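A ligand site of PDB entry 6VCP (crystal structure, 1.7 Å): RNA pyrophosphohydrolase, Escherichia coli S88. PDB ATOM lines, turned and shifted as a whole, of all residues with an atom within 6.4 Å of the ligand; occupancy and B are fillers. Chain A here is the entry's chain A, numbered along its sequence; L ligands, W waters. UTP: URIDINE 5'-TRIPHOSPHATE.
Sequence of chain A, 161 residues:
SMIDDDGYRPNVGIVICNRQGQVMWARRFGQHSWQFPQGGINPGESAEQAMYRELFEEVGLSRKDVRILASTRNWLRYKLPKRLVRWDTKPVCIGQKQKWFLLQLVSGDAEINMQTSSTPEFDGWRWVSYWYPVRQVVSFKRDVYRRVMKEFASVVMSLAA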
ATOM      1  N   ARG A   9      -5.302  10.450  13.048  1.00  0.00           N
ATOM      2  CA  ARG A   9      -4.243   9.854  12.259  1.00  0.00           C
ATOM      3  C   ARG A   9      -4.151   8.345  12.562  1.00  0.00           C
ATOM      4  O   ARG A   9      -4.075   7.970  13.730  1.00  0.00           O
ATOM      5  CB  ARG A   9      -2.946  10.543  12.589  1.00  0.00           C
ATOM      6  CG  ARG A   9      -1.747  10.210  11.780  1.00  0.00           C
ATOM      7  CD  ARG A   9      -0.557  10.984  12.370  1.00  0.00           C
ATOM      8  NE  ARG A   9       0.669  10.763  11.609  1.00  0.00           N
ATOM      9  CZ  ARG A   9       1.732  10.116  12.066  1.00  0.00           C
ATOM     10  NH1 ARG A   9       1.732   9.625  13.311  1.00  0.00           N
ATOM     11  NH2 ARG A   9       2.790   9.967  11.291  1.00  0.00           N
ATOM     12  N   ASN A  11      -2.491   4.912  13.305  1.00  0.00           N
ATOM     13  CA  ASN A  11      -1.198   4.625  13.936  1.00  0.00           C
ATOM     14  C   ASN A  11      -1.215   3.190  14.468  1.00  0.00           C
ATOM     15  O   ASN A  11      -2.269   2.595  14.635  1.00  0.00           O
ATOM     16  CB  ASN A  11      -0.922   5.604  15.089  1.00  0.00           C
ATOM     17  CG  ASN A  11      -0.194   6.870  14.633  1.00  0.00           C
ATOM     18  OD1 ASN A  11       1.028   7.010  14.808  1.00  0.00           O
ATOM     19  ND2 ASN A  11      -0.944   7.809  14.062  1.00  0.00           N
ATOM     20  N   ARG A  28      11.333   8.469  25.376  1.00  0.00           N
ATOM     21  CA  ARG A  28      11.201   9.408  24.257  1.00  0.00           C
ATOM     22  C   ARG A  28      12.479  10.223  24.101  1.00  0.00           C
ATOM     23  O   ARG A  28      13.035  10.711  25.087  1.00  0.00           O
ATOM     24  CB  ARG A  28      10.007  10.331  24.511  1.00  0.00           C
ATOM     25  CG  ARG A  28       8.635   9.670  24.261  1.00  0.00           C
ATOM     26  CD  ARG A  28       7.492  10.630  24.561  1.00  0.00           C
ATOM     27  NE  ARG A  28       7.493  11.742  23.607  1.00  0.00           N
ATOM     28  CZ  ARG A  28       6.811  11.732  22.456  1.00  0.00           C
ATOM     29  NH1 ARG A  28       6.856  12.776  21.615  1.00  0.00           N
ATOM     30  NH2 ARG A  28       6.071  10.686  22.128  1.00  0.00           N
ATOM     31  N   GLN A  31      13.841  13.382  26.180  1.00  0.00           N
ATOM     32  CA  GLN A  31      12.833  13.727  27.184  1.00  0.00           C
ATOM     33  C   GLN A  31      12.993  12.848  28.420  1.00  0.00           C
ATOM     34  O   GLN A  31      13.877  11.972  28.501  1.00  0.00           O
ATOM     35  CB  GLN A  31      11.427  13.600  26.602  1.00  0.00           C
ATOM     36  CG  GLN A  31      11.164  14.434  25.378  1.00  0.00           C
ATOM     37  CD  GLN A  31      11.163  15.932  25.712  1.00  0.00           C
ATOM     38  OE1 GLN A  31      10.846  16.324  26.853  1.00  0.00           O
ATOM     39  NE2 GLN A  31      11.518  16.764  24.737  1.00  0.00           N
ATOM     40  N   SER A  33      10.055  11.352  29.534  1.00  0.00           N
ATOM     41  CA  SER A  33       8.816  10.615  29.404  1.00  0.00           C
ATOM     42  C   SER A  33       9.059   9.377  28.569  1.00  0.00           C
ATOM     43  O   SER A  33       9.958   9.341  27.720  1.00  0.00           O
ATOM     44  CB  SER A  33       7.754  11.484  28.751  1.00  0.00           C
ATOM     45  OG  SER A  33       8.267  12.102  27.587  1.00  0.00           O
ATOM     46  N   TRP A  34       8.280   8.349  28.859  1.00  0.00           N
ATOM     47  CA  TRP A  34       8.498   7.024  28.294  1.00  0.00           C
ATOM     48  C   TRP A  34       7.196   6.518  27.692  1.00  0.00           C
ATOM     49  O   TRP A  34       6.103   6.949  28.058  1.00  0.00           O
ATOM     50  CB  TRP A  34       8.963   6.032  29.362  1.00  0.00           C
ATOM     51  CG  TRP A  34      10.282   6.341  30.011  1.00  0.00           C
ATOM     52  CD1 TRP A  34      10.590   7.468  30.739  1.00  0.00           C
ATOM     53  CD2 TRP A  34      11.457   5.524  30.017  1.00  0.00           C
ATOM     54  NE1 TRP A  34      11.909   7.386  31.203  1.00  0.00           N
ATOM     55  CE2 TRP A  34      12.444   6.201  30.788  1.00  0.00           C
ATOM     56  CE3 TRP A  34      11.767   4.264  29.485  1.00  0.00           C
ATOM     57  CZ2 TRP A  34      13.726   5.671  30.985  1.00  0.00           C
ATOM     58  CZ3 TRP A  34      13.044   3.741  29.693  1.00  0.00           C
ATOM     59  CH2 TRP A  34      13.995   4.454  30.447  1.00  0.00           C
ATOM     60  N   GLN A  35       7.327   5.539  26.790  1.00  0.00           N
ATOM     61  CA  GLN A  35       6.136   5.008  26.113  1.00  0.00           C
ATOM     62  C   GLN A  35       6.486   3.720  25.391  1.00  0.00           C
ATOM     63  O   GLN A  35       7.651   3.324  25.310  1.00  0.00           O
ATOM     64  CB  GLN A  35       5.585   6.023  25.132  1.00  0.00           C
ATOM     65  CG  GLN A  35       6.494   6.190  23.930  1.00  0.00           C
ATOM     66  CD  GLN A  35       5.994   7.224  22.945  1.00  0.00           C
ATOM     67  OE1 GLN A  35       5.523   8.282  23.332  1.00  0.00           O
ATOM     68  NE2 GLN A  35       6.129   6.922  21.655  1.00  0.00           N
ATOM     69  N   GLN A  38       5.364   3.504  18.828  1.00  0.00           N
ATOM     70  CA  GLN A  38       4.178   3.710  18.004  1.00  0.00           C
ATOM     71  C   GLN A  38       4.550   4.522  16.759  1.00  0.00           C
ATOM     72  O   GLN A  38       5.504   5.304  16.752  1.00  0.00           O
ATOM     73  CB  GLN A  38       3.086   4.377  18.811  1.00  0.00           C
ATOM     74  CG  GLN A  38       3.462   5.781  19.244  1.00  0.00           C
ATOM     75  CD  GLN A  38       2.288   6.508  19.834  1.00  0.00           C
ATOM     76  OE1 GLN A  38       1.850   6.196  20.927  1.00  0.00           O
ATOM     77  NE2 GLN A  38       1.784   7.495  19.098  1.00  0.00           N
ATOM     78  N   GLY A  39       3.819   4.274  15.671  1.00  0.00           N
ATOM     79  CA  GLY A  39       4.188   4.925  14.437  1.00  0.00           C
ATOM     80  C   GLY A  39       3.006   5.009  13.499  1.00  0.00           C
ATOM     81  O   GLY A  39       2.011   4.325  13.676  1.00  0.00           O
ATOM     82  N   GLY A  40       3.124   5.893  12.523  1.00  0.00           N
ATOM     83  CA  GLY A  40       2.006   6.107  11.623  1.00  0.00           C
ATOM     84  C   GLY A  40       1.874   5.032  10.580  1.00  0.00           C
ATOM     85  O   GLY A  40       2.804   4.295  10.255  1.00  0.00           O
ATOM     86  N   TYR A  78      -7.106   8.425  21.034  1.00  0.00           N
ATOM     87  CA  TYR A  78      -6.862   9.446  22.043  1.00  0.00           C
ATOM     88  C   TYR A  78      -6.775  10.789  21.349  1.00  0.00           C
ATOM     89  O   TYR A  78      -6.358  10.878  20.179  1.00  0.00           O
ATOM     90  CB  TYR A  78      -5.590   9.180  22.857  1.00  0.00           C
ATOM     91  CG  TYR A  78      -4.263   9.218  22.094  1.00  0.00           C
ATOM     92  CD1 TYR A  78      -3.649  10.415  21.785  1.00  0.00           C
ATOM     93  CD2 TYR A  78      -3.606   8.054  21.790  1.00  0.00           C
ATOM     94  CE1 TYR A  78      -2.425  10.429  21.118  1.00  0.00           C
ATOM     95  CE2 TYR A  78      -2.402   8.066  21.132  1.00  0.00           C
ATOM     96  CZ  TYR A  78      -1.811   9.250  20.802  1.00  0.00           C
ATOM     97  OH  TYR A  78      -0.603   9.264  20.153  1.00  0.00           O
ATOM     98  N   LEU A  80      -5.262  14.720  21.244  1.00  0.00           N
ATOM     99  CA  LEU A  80      -4.174  15.562  21.713  1.00  0.00           C
ATOM    100  C   LEU A  80      -4.717  16.656  22.627  1.00  0.00           C
ATOM    101  O   LEU A  80      -5.813  17.168  22.400  1.00  0.00           O
ATOM    102  CB  LEU A  80      -3.454  16.207  20.531  1.00  0.00           C
ATOM    103  CG  LEU A  80      -2.783  15.249  19.570  1.00  0.00           C
ATOM    104  CD1 LEU A  80      -2.290  16.013  18.341  1.00  0.00           C
ATOM    105  CD2 LEU A  80      -1.639  14.571  20.315  1.00  0.00           C
ATOM    106  N   PRO A  81      -3.962  17.040  23.656  1.00  0.00           N
ATOM    107  CA  PRO A  81      -4.313  18.249  24.400  1.00  0.00           C
ATOM    108  C   PRO A  81      -4.479  19.408  23.427  1.00  0.00           C
ATOM    109  O   PRO A  81      -3.764  19.493  22.422  1.00  0.00           O
ATOM    110  CB  PRO A  81      -3.120  18.458  25.332  1.00  0.00           C
ATOM    111  CG  PRO A  81      -2.564  17.057  25.518  1.00  0.00           C
ATOM    112  CD  PRO A  81      -2.752  16.394  24.185  1.00  0.00           C
ATOM    113  N   LEU A  84      -1.650  21.293  21.929  1.00  0.00           N
ATOM    114  CA  LEU A  84      -0.709  20.546  21.097  1.00  0.00           C
ATOM    115  C   LEU A  84      -1.248  20.240  19.707  1.00  0.00           C
ATOM    116  O   LEU A  84      -0.562  19.570  18.930  1.00  0.00           O
ATOM    117  CB  LEU A  84      -0.312  19.238  21.786  1.00  0.00           C
ATOM    118  CG  LEU A  84       0.792  19.248  22.856  1.00  0.00           C
ATOM    119  CD1 LEU A  84       0.573  20.332  23.913  1.00  0.00           C
ATOM    120  CD2 LEU A  84       0.882  17.891  23.523  1.00  0.00           C
ATOM    121  N   GLN A  96      -4.845  10.462  17.539  1.00  0.00           N
ATOM    122  CA  GLN A  96      -4.496   9.269  16.804  1.00  0.00           C
ATOM    123  C   GLN A  96      -5.520   8.167  17.051  1.00  0.00           C
ATOM    124  O   GLN A  96      -6.111   8.071  18.141  1.00  0.00           O
ATOM    125  CB  GLN A  96      -3.106   8.756  17.174  1.00  0.00           C
ATOM    126  CG  GLN A  96      -2.011   9.732  16.851  1.00  0.00           C
ATOM    127  CD  GLN A  96      -0.654   9.114  17.040  1.00  0.00           C
ATOM    128  OE1 GLN A  96      -0.537   7.885  17.255  1.00  0.00           O
ATOM    129  NE2 GLN A  96       0.383   9.936  16.963  1.00  0.00           N
ATOM    130  N   GLU A 121      13.246   7.822  17.552  1.00  0.00           N
ATOM    131  CA  GLU A 121      12.064   7.974  18.392  1.00  0.00           C
ATOM    132  C   GLU A 121      12.451   7.894  19.851  1.00  0.00           C
ATOM    133  O   GLU A 121      11.846   8.561  20.706  1.00  0.00           O
ATOM    134  CB  GLU A 121      11.005   6.920  18.024  1.00  0.00           C
ATOM    135  CG  GLU A 121       9.743   6.860  18.944  1.00  0.00           C
ATOM    136  CD  GLU A 121       8.768   5.737  18.570  1.00  0.00           C
ATOM    137  OE1 GLU A 121       9.134   4.967  17.656  1.00  0.00           O
ATOM    138  OE2 GLU A 121       7.673   5.605  19.191  1.00  0.00           O
ATOM    139  N   VAL A 137       2.713   6.404  31.466  1.00  0.00           N
ATOM    140  CA  VAL A 137       2.586   7.107  30.196  1.00  0.00           C
ATOM    141  C   VAL A 137       1.951   8.478  30.423  1.00  0.00           C
ATOM    142  O   VAL A 137       1.271   8.715  31.427  1.00  0.00           O
ATOM    143  CB  VAL A 137       1.774   6.255  29.206  1.00  0.00           C
ATOM    144  CG1 VAL A 137       0.342   6.156  29.683  1.00  0.00           C
ATOM    145  CG2 VAL A 137       1.913   6.761  27.751  1.00  0.00           C
ATOM    146  N   VAL A 138       2.181   9.381  29.461  1.00  0.00           N
ATOM    147  CA  VAL A 138       1.572  10.710  29.509  1.00  0.00           C
ATOM    148  C   VAL A 138       0.047  10.572  29.677  1.00  0.00           C
ATOM    149  O   VAL A 138      -0.579   9.655  29.130  1.00  0.00           O
ATOM    150  CB  VAL A 138       1.958  11.513  28.248  1.00  0.00           C
ATOM    151  CG1 VAL A 138       1.344  10.934  26.987  1.00  0.00           C
ATOM    152  CG2 VAL A 138       1.594  13.029  28.409  1.00  0.00           C
ATOM    153  N   PHE A 140      -2.711  11.860  28.688  1.00  0.00           N
ATOM    154  CA  PHE A 140      -3.745  11.769  27.655  1.00  0.00           C
ATOM    155  C   PHE A 140      -3.749  10.439  26.895  1.00  0.00           C
ATOM    156  O   PHE A 140      -4.684  10.195  26.108  1.00  0.00           O
ATOM    157  CB  PHE A 140      -3.687  12.948  26.658  1.00  0.00           C
ATOM    158  CG  PHE A 140      -2.392  13.063  25.844  1.00  0.00           C
ATOM    159  CD1 PHE A 140      -2.255  12.398  24.618  1.00  0.00           C
ATOM    160  CD2 PHE A 140      -1.333  13.857  26.282  1.00  0.00           C
ATOM    161  CE1 PHE A 140      -1.087  12.507  23.871  1.00  0.00           C
ATOM    162  CE2 PHE A 140      -0.160  13.959  25.523  1.00  0.00           C
ATOM    163  CZ  PHE A 140      -0.045  13.284  24.310  1.00  0.00           C
ATOM    164  N   LYS A 141      -2.746   9.582  27.111  1.00  0.00           N
ATOM    165  CA  LYS A 141      -2.758   8.242  26.548  1.00  0.00           C
ATOM    166  C   LYS A 141      -3.165   7.178  27.574  1.00  0.00           C
ATOM    167  O   LYS A 141      -3.233   6.002  27.227  1.00  0.00           O
ATOM    168  CB  LYS A 141      -1.376   7.888  25.980  1.00  0.00           C
ATOM    169  CG  LYS A 141      -0.893   8.761  24.827  1.00  0.00           C
ATOM    170  CD  LYS A 141       0.385   8.183  24.208  1.00  0.00           C
ATOM    171  CE  LYS A 141       0.981   9.122  23.190  1.00  0.00           C
ATOM    172  NZ  LYS A 141       2.236   8.604  22.565  1.00  0.00           N
HETATM  173  PA  UTP L   1       2.272  11.632  20.110  1.00  0.00           P
HETATM  174  O1A UTP L   1       2.917  10.546  20.913  1.00  0.00           O
HETATM  175  O2A UTP L   1       0.760  11.485  19.949  1.00  0.00           O
HETATM  176  O3A UTP L   1       2.973  11.758  18.628  1.00  0.00           O
HETATM  177  O5' UTP L   1       2.605  12.967  20.906  1.00  0.00           O
HETATM  178  PB  UTP L   1       4.497  12.137  18.170  1.00  0.00           P
HETATM  179  O1B UTP L   1       4.556  13.672  17.953  1.00  0.00           O
HETATM  180  O2B UTP L   1       5.466  11.831  19.272  1.00  0.00           O
HETATM  181  O3B UTP L   1       4.918  11.302  16.812  1.00  0.00           O
HETATM  182  PG  UTP L   1       4.130  10.221  15.930  1.00  0.00           P
HETATM  183  O1G UTP L   1       3.793   8.985  16.760  1.00  0.00           O
HETATM  184  O2G UTP L   1       5.011   9.809  14.753  1.00  0.00           O
HETATM  185  O3G UTP L   1       2.873  10.926  15.462  1.00  0.00           O
HETATM  186  C5' UTP L   1       2.037  14.207  20.466  1.00  0.00           C
HETATM  187  C4' UTP L   1       2.768  15.317  21.241  1.00  0.00           C
HETATM  188  O4' UTP L   1       2.537  15.167  22.639  1.00  0.00           O
HETATM  189  C1' UTP L   1       3.668  15.621  23.363  1.00  0.00           C
HETATM  190  C2' UTP L   1       4.799  15.906  22.360  1.00  0.00           C
HETATM  191  O2' UTP L   1       4.859  17.322  22.151  1.00  0.00           O
HETATM  192  C3' UTP L   1       4.285  15.212  21.097  1.00  0.00           C
HETATM  193  O3' UTP L   1       4.765  15.852  19.908  1.00  0.00           O
HETATM  194  N1  UTP L   1       4.074  14.554  24.308  1.00  0.00           N
HETATM  195  C6  UTP L   1       3.868  13.194  23.790  1.00  0.00           C
HETATM  196  C2  UTP L   1       4.513  14.912  25.537  1.00  0.00           C
HETATM  197  O2  UTP L   1       4.641  16.080  25.905  1.00  0.00           O
HETATM  198  N3  UTP L   1       4.853  13.924  26.388  1.00  0.00           N
HETATM  199  C4  UTP L   1       4.778  12.575  26.159  1.00  0.00           C
HETATM  200  O4  UTP L   1       5.111  11.760  27.022  1.00  0.00           O
HETATM  201  C5  UTP L   1       4.278  12.156  24.816  1.00  0.00           C
HETATM  202  O   HOH W   1       3.735   8.871  24.887  1.00  0.00           O
HETATM  203  O   HOH W   2       4.542   9.088  27.690  1.00  0.00           O
HETATM  204  O   HOH W   3       7.102  17.142  26.743  1.00  0.00           O
HETATM  205  O   HOH W   4       7.822  10.483  18.857  1.00  0.00           O
HETATM  206  O   HOH W   5       6.350   7.720  16.897  1.00  0.00           O
HETATM  207  O   HOH W   6       4.821   8.696  19.919  1.00  0.00           O
HETATM  208  O   HOH W   7       0.246  12.887  17.478  1.00  0.00           O
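NH1 of Arg 28 lies within salt-bridge range of O2B of the ligand (2.9 Å). The side-chain amide nitrogen (NE2) of Gln 38 sits at hydrogen-bond distance from an oxygen (O1G) of the ligand. OG of Ser 33 sits close to O4 of the ligand. The side-chain amino group of Lys 141 is in salt-bridge range of an oxygen (O1A) of the ligand. The guanidinium group (NH1) of Arg 9 is in salt-bridge range of an oxygen (O3G) of the ligand (2.8 Å). NE2 of Gln 96 is in hydrogen-bond range of O3G of the ligand (3.1 Å). The side-chain hydroxyl (OH) of Tyr 78 is in hydrogen-bond range of an oxygen (O2A) of the ligand.
The side-chain hydroxyl (OH) of Tyr 78 is in hydrogen-bond range of the side-chain amide nitrogen (NE2) of Gln 38, 3.2 Å away. N of Arg 28 is in hydrogen-bond range of O of Ser 33, 2.9 Å away. The backbone NH (N) of Gly 40 sits at hydrogen-bond distance from the side-chain amide oxygen (OD1) of Asn 11 (3.3 Å). The side-chain amide oxygen (OE1) of Gln 96 lies close to the side-chain amide oxygen (OD1) of Asn 11, at 3.0 Å. The side-chain amino group (NZ) of Lys 141 is in hydrogen-bond range of the side-chain amide oxygen (OE1) of Gln 38, 2.9 Å away. The side-chain amino group (NZ) of Lys 141 lies within hydrogen-bond range of the side-chain amide oxygen (OE1) of Gln 35. O of Tyr 78 sits at hydrogen-bond distance from N of Gln 96. N of Gln 38 lies within hydrogen-bond range of OE2 of Glu 121 (3.1 Å).
Residues that only touch the ligand: Asn 11 (3.9 Å), Leu 80 (3.7 Å), Leu 84 (3.3 Å), Val 138 (3.4 Å) and Phe 140 (3.6 Å). Hydrophobic or aromatic side chains that line the ligand: Tyr 78, Leu 80, Leu 84, Val 138 and Phe 140. Within 4 Å of the ligand: Arg 9, Asn 11, Arg 28, Ser 33, Gln 38, Tyr 78, Leu 80, Leu 84, Gln 96, Val 138, Phe 140 and Lys 141. The nearest printed residue that does not touch the ligand is Gln 35 (4.2 Å).
Water W2 lies within hydrogen-bond range of O of Trp 34 (2.7 Å), O4 of the ligand (2.8 Å) and N of Val 138 (3.0 Å). Water W5 lies within hydrogen-bond range of O of Gln 38 (2.6 Å), O1G of the ligand (2.9 Å) and OE2 of Glu 121 (3.4 Å). Water W7 lies within hydrogen-bond range of O2A of the ligand (2.9 Å) and NE2 of Gln 96 (3.0 Å). Water W1 bridges OE1 of Gln 35 and NZ of Lys 141.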
